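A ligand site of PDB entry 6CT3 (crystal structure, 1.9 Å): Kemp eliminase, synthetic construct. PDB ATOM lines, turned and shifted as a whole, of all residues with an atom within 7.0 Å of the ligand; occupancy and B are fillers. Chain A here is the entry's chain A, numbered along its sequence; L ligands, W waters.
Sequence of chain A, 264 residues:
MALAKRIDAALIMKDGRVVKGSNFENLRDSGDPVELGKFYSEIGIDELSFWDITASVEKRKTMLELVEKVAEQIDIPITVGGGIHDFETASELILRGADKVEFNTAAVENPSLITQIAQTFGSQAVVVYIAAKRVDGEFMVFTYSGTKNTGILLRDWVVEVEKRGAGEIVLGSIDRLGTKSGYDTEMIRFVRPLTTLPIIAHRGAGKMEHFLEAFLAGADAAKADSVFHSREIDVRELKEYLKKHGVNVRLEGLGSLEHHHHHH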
ATOM      1  N   ALA A   9      -1.309   1.255 -28.070  1.00  0.00           N
ATOM      2  CA  ALA A   9      -1.656  -0.150 -28.339  1.00  0.00           C
ATOM      3  C   ALA A   9      -2.177  -0.716 -27.032  1.00  0.00           C
ATOM      4  O   ALA A   9      -1.604  -0.469 -25.975  1.00  0.00           O
ATOM      5  CB  ALA A   9      -0.428  -0.932 -28.785  1.00  0.00           C
ATOM      6  N   ALA A  10      -3.184  -1.571 -27.132  1.00  0.00           N
ATOM      7  CA  ALA A  10      -3.755  -2.296 -25.985  1.00  0.00           C
ATOM      8  C   ALA A  10      -3.430  -3.760 -26.117  1.00  0.00           C
ATOM      9  O   ALA A  10      -3.474  -4.282 -27.215  1.00  0.00           O
ATOM     10  CB  ALA A  10      -5.248  -2.134 -25.990  1.00  0.00           C
ATOM     11  N   LEU A  11      -3.056  -4.376 -25.006  1.00  0.00           N
ATOM     12  CA  LEU A  11      -2.765  -5.752 -24.924  1.00  0.00           C
ATOM     13  C   LEU A  11      -3.657  -6.332 -23.826  1.00  0.00           C
ATOM     14  O   LEU A  11      -3.665  -5.850 -22.682  1.00  0.00           O
ATOM     15  CB  LEU A  11      -1.280  -5.937 -24.560  1.00  0.00           C
ATOM     16  CG  LEU A  11      -0.167  -5.482 -25.542  1.00  0.00           C
ATOM     17  CD1 LEU A  11       0.132  -3.986 -25.530  1.00  0.00           C
ATOM     18  CD2 LEU A  11       1.160  -6.127 -25.233  1.00  0.00           C
ATOM     19  N   ILE A  12      -4.321  -7.442 -24.124  1.00  0.00           N
ATOM     20  CA  ILE A  12      -5.063  -8.215 -23.114  1.00  0.00           C
ATOM     21  C   ILE A  12      -4.132  -9.274 -22.523  1.00  0.00           C
ATOM     22  O   ILE A  12      -3.489 -10.024 -23.267  1.00  0.00           O
ATOM     23  CB  ILE A  12      -6.293  -8.936 -23.740  1.00  0.00           C
ATOM     24  CG1 ILE A  12      -7.286  -7.934 -24.406  1.00  0.00           C
ATOM     25  CG2 ILE A  12      -7.018  -9.758 -22.688  1.00  0.00           C
ATOM     26  CD1 ILE A  12      -8.127  -8.585 -25.456  1.00  0.00           C
ATOM     27  N   SER A  49      -0.934  -0.110 -23.208  1.00  0.00           N
ATOM     28  CA  SER A  49      -1.776  -0.475 -22.057  1.00  0.00           C
ATOM     29  C   SER A  49      -1.922  -1.986 -21.976  1.00  0.00           C
ATOM     30  O   SER A  49      -2.073  -2.662 -23.007  1.00  0.00           O
ATOM     31  CB  SER A  49      -3.138   0.218 -22.105  1.00  0.00           C
ATOM     32  OG  SER A  49      -3.913  -0.207 -23.209  1.00  0.00           O
ATOM     33  N   PHE A  50      -1.855  -2.482 -20.759  1.00  0.00           N
ATOM     34  CA  PHE A  50      -2.114  -3.869 -20.446  1.00  0.00           C
ATOM     35  C   PHE A  50      -3.408  -3.940 -19.660  1.00  0.00           C
ATOM     36  O   PHE A  50      -3.571  -3.188 -18.669  1.00  0.00           O
ATOM     37  CB  PHE A  50      -0.966  -4.384 -19.588  1.00  0.00           C
ATOM     38  CG  PHE A  50       0.390  -4.354 -20.327  1.00  0.00           C
ATOM     39  CD1 PHE A  50       1.212  -3.226 -20.267  1.00  0.00           C
ATOM     40  CD2 PHE A  50       0.797  -5.437 -21.117  1.00  0.00           C
ATOM     41  CE1 PHE A  50       2.466  -3.197 -20.928  1.00  0.00           C
ATOM     42  CE2 PHE A  50       2.043  -5.432 -21.745  1.00  0.00           C
ATOM     43  CZ  PHE A  50       2.879  -4.305 -21.686  1.00  0.00           C
ATOM     44  N   TRP A  51      -4.307  -4.822 -20.054  1.00  0.00           N
ATOM     45  CA  TRP A  51      -5.557  -5.067 -19.380  1.00  0.00           C
ATOM     46  C   TRP A  51      -5.598  -6.528 -18.971  1.00  0.00           C
ATOM     47  O   TRP A  51      -5.727  -7.377 -19.764  1.00  0.00           O
ATOM     48  CB  TRP A  51      -6.765  -4.770 -20.216  1.00  0.00           C
ATOM     49  CG  TRP A  51      -8.028  -4.579 -19.420  1.00  0.00           C
ATOM     50  CD1 TRP A  51      -8.264  -3.616 -18.522  1.00  0.00           C
ATOM     51  CD2 TRP A  51      -9.187  -5.369 -19.463  1.00  0.00           C
ATOM     52  NE1 TRP A  51      -9.475  -3.757 -17.986  1.00  0.00           N
ATOM     53  CE2 TRP A  51     -10.080  -4.832 -18.558  1.00  0.00           C
ATOM     54  CE3 TRP A  51      -9.561  -6.458 -20.199  1.00  0.00           C
ATOM     55  CZ2 TRP A  51     -11.318  -5.326 -18.371  1.00  0.00           C
ATOM     56  CZ3 TRP A  51     -10.802  -6.965 -20.019  1.00  0.00           C
ATOM     57  CH2 TRP A  51     -11.671  -6.412 -19.106  1.00  0.00           C
ATOM     58  N   ILE A  53      -6.978  -9.888 -17.431  1.00  0.00           N
ATOM     59  CA  ILE A  53      -8.145 -10.683 -17.117  1.00  0.00           C
ATOM     60  C   ILE A  53      -7.860 -11.966 -16.290  1.00  0.00           C
ATOM     61  O   ILE A  53      -8.687 -12.821 -16.255  1.00  0.00           O
ATOM     62  CB  ILE A  53      -8.861 -11.069 -18.392  1.00  0.00           C
ATOM     63  CG1 ILE A  53      -8.013 -12.010 -19.245  1.00  0.00           C
ATOM     64  CG2 ILE A  53      -9.198  -9.813 -19.198  1.00  0.00           C
ATOM     65  CD1 ILE A  53      -8.726 -12.591 -20.439  1.00  0.00           C
ATOM     66  N   THR A  79       0.693   1.636 -19.172  1.00  0.00           N
ATOM     67  CA  THR A  79      -0.474   1.705 -18.338  1.00  0.00           C
ATOM     68  C   THR A  79      -0.871   0.276 -17.979  1.00  0.00           C
ATOM     69  O   THR A  79      -0.879  -0.617 -18.817  1.00  0.00           O
ATOM     70  CB  THR A  79      -1.620   2.436 -19.007  1.00  0.00           C
ATOM     71  OG1 THR A  79      -1.281   3.798 -19.356  1.00  0.00           O
ATOM     72  CG2 THR A  79      -2.794   2.511 -18.057  1.00  0.00           C
ATOM     73  N   GLY A  81      -3.975  -2.038 -15.991  1.00  0.00           N
ATOM     74  CA  GLY A  81      -5.356  -2.090 -15.499  1.00  0.00           C
ATOM     75  C   GLY A  81      -6.018  -3.488 -15.562  1.00  0.00           C
ATOM     76  O   GLY A  81      -5.446  -4.463 -16.095  1.00  0.00           O
ATOM     77  N   GLY A  82      -7.193  -3.578 -15.011  1.00  0.00           N
ATOM     78  CA  GLY A  82      -8.023  -4.801 -15.007  1.00  0.00           C
ATOM     79  C   GLY A  82      -8.149  -5.269 -13.617  1.00  0.00           C
ATOM     80  O   GLY A  82      -7.251  -5.912 -13.093  1.00  0.00           O
ATOM     81  N   GLU A 102      -4.947   2.306 -14.531  1.00  0.00           N
ATOM     82  CA  GLU A 102      -6.229   2.516 -15.130  1.00  0.00           C
ATOM     83  C   GLU A 102      -7.348   1.900 -14.286  1.00  0.00           C
ATOM     84  O   GLU A 102      -7.234   0.821 -13.839  1.00  0.00           O
ATOM     85  CB  GLU A 102      -6.178   1.929 -16.520  1.00  0.00           C
ATOM     86  CG  GLU A 102      -7.416   1.837 -17.340  1.00  0.00           C
ATOM     87  CD  GLU A 102      -7.148   1.303 -18.771  1.00  0.00           C
ATOM     88  OE1 GLU A 102      -7.297   0.119 -19.028  1.00  0.00           O
ATOM     89  OE2 GLU A 102      -6.767   2.028 -19.658  1.00  0.00           O
ATOM     90  N   ASN A 104     -11.642   1.627 -13.634  1.00  0.00           N
ATOM     91  CA  ASN A 104     -12.984   1.808 -14.112  1.00  0.00           C
ATOM     92  C   ASN A 104     -13.943   1.543 -12.966  1.00  0.00           C
ATOM     93  O   ASN A 104     -14.353   2.477 -12.275  1.00  0.00           O
ATOM     94  CB  ASN A 104     -13.265   0.915 -15.322  1.00  0.00           C
ATOM     95  CG  ASN A 104     -14.697   1.087 -15.849  1.00  0.00           C
ATOM     96  OD1 ASN A 104     -15.525   1.885 -15.317  1.00  0.00           O
ATOM     97  ND2 ASN A 104     -14.982   0.371 -16.889  1.00  0.00           N
ATOM     98  N   VAL A 127      -5.358   7.043 -14.915  1.00  0.00           N
ATOM     99  CA  VAL A 127      -6.198   7.013 -16.098  1.00  0.00           C
ATOM    100  C   VAL A 127      -7.539   6.418 -15.637  1.00  0.00           C
ATOM    101  O   VAL A 127      -7.536   5.371 -14.970  1.00  0.00           O
ATOM    102  CB  VAL A 127      -5.613   6.041 -17.112  1.00  0.00           C
ATOM    103  CG1 VAL A 127      -6.536   5.914 -18.300  1.00  0.00           C
ATOM    104  CG2 VAL A 127      -4.246   6.563 -17.578  1.00  0.00           C
ATOM    105  N   TYR A 129     -10.798   4.726 -17.217  1.00  0.00           N
ATOM    106  CA  TYR A 129     -11.453   4.156 -18.417  1.00  0.00           C
ATOM    107  C   TYR A 129     -12.975   4.262 -18.193  1.00  0.00           C
ATOM    108  O   TYR A 129     -13.534   3.779 -17.192  1.00  0.00           O
ATOM    109  CB  TYR A 129     -11.014   2.701 -18.567  1.00  0.00           C
ATOM    110  CG  TYR A 129     -11.461   2.077 -19.863  1.00  0.00           C
ATOM    111  CD1 TYR A 129     -12.819   1.679 -20.065  1.00  0.00           C
ATOM    112  CD2 TYR A 129     -10.566   1.857 -20.887  1.00  0.00           C
ATOM    113  CE1 TYR A 129     -13.225   1.111 -21.264  1.00  0.00           C
ATOM    114  CE2 TYR A 129     -10.987   1.269 -22.074  1.00  0.00           C
ATOM    115  CZ  TYR A 129     -12.310   0.913 -22.243  1.00  0.00           C
ATOM    116  OH  TYR A 129     -12.660   0.411 -23.477  1.00  0.00           O
ATOM    117  N   ILE A 130     -13.656   4.943 -19.090  1.00  0.00           N
ATOM    118  CA  ILE A 130     -15.143   5.076 -19.054  1.00  0.00           C
ATOM    119  C   ILE A 130     -15.721   4.289 -20.197  1.00  0.00           C
ATOM    120  O   ILE A 130     -15.494   4.564 -21.427  1.00  0.00           O
ATOM    121  CB  ILE A 130     -15.605   6.522 -19.145  1.00  0.00           C
ATOM    122  CG1 ILE A 130     -14.904   7.385 -18.109  1.00  0.00           C
ATOM    123  CG2 ILE A 130     -17.103   6.604 -18.943  1.00  0.00           C
ATOM    124  CD1 ILE A 130     -15.162   8.859 -18.298  1.00  0.00           C
ATOM    125  N   ALA A 131     -16.403   3.211 -19.815  1.00  0.00           N
ATOM    126  CA  ALA A 131     -17.123   2.391 -20.773  1.00  0.00           C
ATOM    127  C   ALA A 131     -18.557   2.912 -20.853  1.00  0.00           C
ATOM    128  O   ALA A 131     -19.266   2.854 -19.859  1.00  0.00           O
ATOM    129  CB  ALA A 131     -17.136   0.908 -20.330  1.00  0.00           C
ATOM    130  N   TYR A 144     -18.119  -3.344 -14.484  1.00  0.00           N
ATOM    131  CA  TYR A 144     -17.959  -4.795 -14.530  1.00  0.00           C
ATOM    132  C   TYR A 144     -17.838  -5.309 -15.972  1.00  0.00           C
ATOM    133  O   TYR A 144     -18.648  -6.127 -16.423  1.00  0.00           O
ATOM    134  CB  TYR A 144     -19.076  -5.492 -13.716  1.00  0.00           C
ATOM    135  CG  TYR A 144     -18.999  -5.140 -12.233  1.00  0.00           C
ATOM    136  CD1 TYR A 144     -18.158  -5.828 -11.385  1.00  0.00           C
ATOM    137  CD2 TYR A 144     -19.718  -4.065 -11.727  1.00  0.00           C
ATOM    138  CE1 TYR A 144     -18.055  -5.486 -10.031  1.00  0.00           C
ATOM    139  CE2 TYR A 144     -19.621  -3.698 -10.405  1.00  0.00           C
ATOM    140  CZ  TYR A 144     -18.811  -4.408  -9.568  1.00  0.00           C
ATOM    141  OH  TYR A 144     -18.707  -4.003  -8.305  1.00  0.00           O
ATOM    142  N   SER A 145     -16.856  -4.826 -16.704  1.00  0.00           N
ATOM    143  CA  SER A 145     -16.641  -5.150 -18.139  1.00  0.00           C
ATOM    144  C   SER A 145     -17.881  -5.035 -19.033  1.00  0.00           C
ATOM    145  O   SER A 145     -18.215  -5.965 -19.767  1.00  0.00           O
ATOM    146  CB  SER A 145     -16.007  -6.526 -18.282  1.00  0.00           C
ATOM    147  OG  SER A 145     -14.872  -6.675 -17.416  1.00  0.00           O
ATOM    148  N   GLY A 146     -18.569  -3.893 -18.965  1.00  0.00           N
ATOM    149  CA  GLY A 146     -19.695  -3.660 -19.844  1.00  0.00           C
ATOM    150  C   GLY A 146     -20.989  -4.280 -19.395  1.00  0.00           C
ATOM    151  O   GLY A 146     -21.939  -4.262 -20.138  1.00  0.00           O
ATOM    152  N   VAL A 170      -9.905   7.361 -20.970  1.00  0.00           N
ATOM    153  CA  VAL A 170     -10.144   6.479 -22.106  1.00  0.00           C
ATOM    154  C   VAL A 170     -11.608   6.328 -22.305  1.00  0.00           C
ATOM    155  O   VAL A 170     -12.328   5.964 -21.366  1.00  0.00           O
ATOM    156  CB  VAL A 170      -9.548   5.076 -21.903  1.00  0.00           C
ATOM    157  CG1 VAL A 170      -9.630   4.301 -23.232  1.00  0.00           C
ATOM    158  CG2 VAL A 170      -8.121   5.200 -21.437  1.00  0.00           C
ATOM    159  N   HIS A 202     -11.390   4.539 -27.803  1.00  0.00           N
ATOM    160  CA  HIS A 202     -11.253   3.081 -27.875  1.00  0.00           C
ATOM    161  C   HIS A 202     -12.490   2.380 -28.412  1.00  0.00           C
ATOM    162  O   HIS A 202     -13.626   2.726 -28.065  1.00  0.00           O
ATOM    163  CB  HIS A 202     -10.887   2.546 -26.464  1.00  0.00           C
ATOM    164  CG  HIS A 202     -10.461   1.120 -26.419  1.00  0.00           C
ATOM    165  ND1 HIS A 202     -10.809   0.281 -25.365  1.00  0.00           N
ATOM    166  CD2 HIS A 202      -9.670   0.400 -27.249  1.00  0.00           C
ATOM    167  CE1 HIS A 202     -10.202  -0.887 -25.548  1.00  0.00           C
ATOM    168  NE2 HIS A 202      -9.565  -0.863 -26.705  1.00  0.00           N
ATOM    169  N   ARG A 203     -12.230   1.290 -29.161  1.00  0.00           N
ATOM    170  CA  ARG A 203     -13.241   0.446 -29.816  1.00  0.00           C
ATOM    171  C   ARG A 203     -13.707   0.972 -31.208  1.00  0.00           C
ATOM    172  O   ARG A 203     -14.179   2.129 -31.357  1.00  0.00           O
ATOM    173  CB  ARG A 203     -14.427   0.118 -28.982  1.00  0.00           C
ATOM    174  CG  ARG A 203     -14.112  -0.484 -27.583  1.00  0.00           C
ATOM    175  CD  ARG A 203     -13.275  -1.757 -27.753  1.00  0.00           C
ATOM    176  NE  ARG A 203     -13.226  -2.531 -26.520  1.00  0.00           N
ATOM    177  CZ  ARG A 203     -12.378  -3.515 -26.272  1.00  0.00           C
ATOM    178  NH1 ARG A 203     -11.466  -3.860 -27.134  1.00  0.00           N
ATOM    179  NH2 ARG A 203     -12.448  -4.151 -25.148  1.00  0.00           N
ATOM    180  N   LYS A 223      -6.574   4.220 -29.376  1.00  0.00           N
ATOM    181  CA  LYS A 223      -6.065   3.008 -28.863  1.00  0.00           C
ATOM    182  C   LYS A 223      -6.651   1.883 -29.718  1.00  0.00           C
ATOM    183  O   LYS A 223      -7.840   1.884 -30.031  1.00  0.00           O
ATOM    184  CB  LYS A 223      -6.566   2.846 -27.428  1.00  0.00           C
ATOM    185  CG  LYS A 223      -5.893   1.697 -26.680  1.00  0.00           C
ATOM    186  CD  LYS A 223      -6.731   1.276 -25.468  1.00  0.00           C
ATOM    187  CE  LYS A 223      -6.514   2.207 -24.329  1.00  0.00           C
ATOM    188  NZ  LYS A 223      -5.355   1.768 -23.545  1.00  0.00           N
ATOM    189  N   ASP A 225      -5.793  -2.706 -30.697  1.00  0.00           N
ATOM    190  CA  ASP A 225      -4.998  -3.903 -30.423  1.00  0.00           C
ATOM    191  C   ASP A 225      -4.689  -4.751 -31.643  1.00  0.00           C
ATOM    192  O   ASP A 225      -3.529  -4.857 -32.059  1.00  0.00           O
ATOM    193  CB  ASP A 225      -5.682  -4.756 -29.353  1.00  0.00           C
ATOM    194  CG  ASP A 225      -4.975  -6.079 -29.121  1.00  0.00           C
ATOM    195  OD1 ASP A 225      -3.793  -6.195 -29.507  1.00  0.00           O
ATOM    196  OD2 ASP A 225      -5.595  -6.986 -28.528  1.00  0.00           O
HETATM  197  N1  LIG L   1      -7.023  -0.113 -21.539  1.00  0.00           N
HETATM  198  C1  LIG L   1      -7.830  -0.899 -21.660  1.00  0.00           C
HETATM  199  C2  LIG L   1      -8.857  -1.897 -21.820  1.00  0.00           C
HETATM  200  C3  LIG L   1      -9.994  -1.814 -20.990  1.00  0.00           C
HETATM  201  C4  LIG L   1      -8.753  -2.935 -22.767  1.00  0.00           C
HETATM  202  O1  LIG L   1      -7.639  -2.990 -23.550  1.00  0.00           O
HETATM  203  C5  LIG L   1      -9.775  -3.895 -22.909  1.00  0.00           C
HETATM  204  C6  LIG L   1     -10.904  -3.802 -22.085  1.00  0.00           C
HETATM  205  C7  LIG L   1     -11.028  -2.764 -21.116  1.00  0.00           C
HETATM  206  N2  LIG L   1     -12.113  -2.700 -20.329  1.00  0.00           N
HETATM  207  O2  LIG L   1     -12.237  -1.667 -19.351  1.00  0.00           O
HETATM  208  O3  LIG L   1     -13.168  -3.663 -20.438  1.00  0.00           O
HETATM  209  O   HOH W   1     -10.840  -2.050 -16.347  1.00  0.00           O
HETATM  210  O   HOH W   2      -5.095  -0.898 -19.315  1.00  0.00           O
HETATM  211  O   HOH W   3     -14.502  -2.130 -18.405  1.00  0.00           O
HETATM  212  O   HOH W   4      -5.207  -2.517 -22.637  1.00  0.00           O
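Water W3 bridges an oxygen (O2) of the ligand and the side-chain amide nitrogen (ND2) of Asn 104.
Water W4 lies within hydrogen-bond range of O1 of the ligand (2.6 Å) and OG of Ser 49 (2.7 Å).
Water W1 lies within hydrogen-bond range of NE1 of Trp 51 and O2 of the ligand.
OE1 of Glu 102 is in hydrogen-bond range of N1 of the ligand (2.5 Å).
The side-chain amino group (NZ) of Lys 223 is in hydrogen-bond range of a nitrogen (N1) of the ligand (3.2 Å).
Ala 10 touches the ligand.
Ser 49 touches the ligand.
Trp 51 touches the ligand.
Tyr 129 touches the ligand.
His 202 touches the ligand (CE1 to C4, 3.7 Å).
Arg 203 touches the ligand (NH2 to C6, 3.4 Å).
Hydrophobic or aromatic side chains that line the ligand: Ala 10, Trp 51, Tyr 129 and His 202.
Of the 25 residues printed, 8 come within 4 Å of the ligand.
N of Leu 11 is in hydrogen-bond range of O of Ser 49 (2.8 Å).
The backbone NH of Trp 51 sits at hydrogen-bond distance from the backbone carbonyl oxygen of Leu 11, 2.9 Å away.
N of Ser 49 is in hydrogen-bond range of O of Ala 9.
A ring nitrogen (ND1) of His 202 is in hydrogen-bond range of the side-chain hydroxyl (OH) of Tyr 129 (2.6 Å).
The backbone carbonyl oxygen (O) of Tyr 129 sits close to the side-chain amide oxygen (OD1) of Asn 104 (3.3 Å).
The side-chain amino group of Lys 223 lies within hydrogen-bond range of the side-chain hydroxyl of Ser 49 (2.5 Å).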
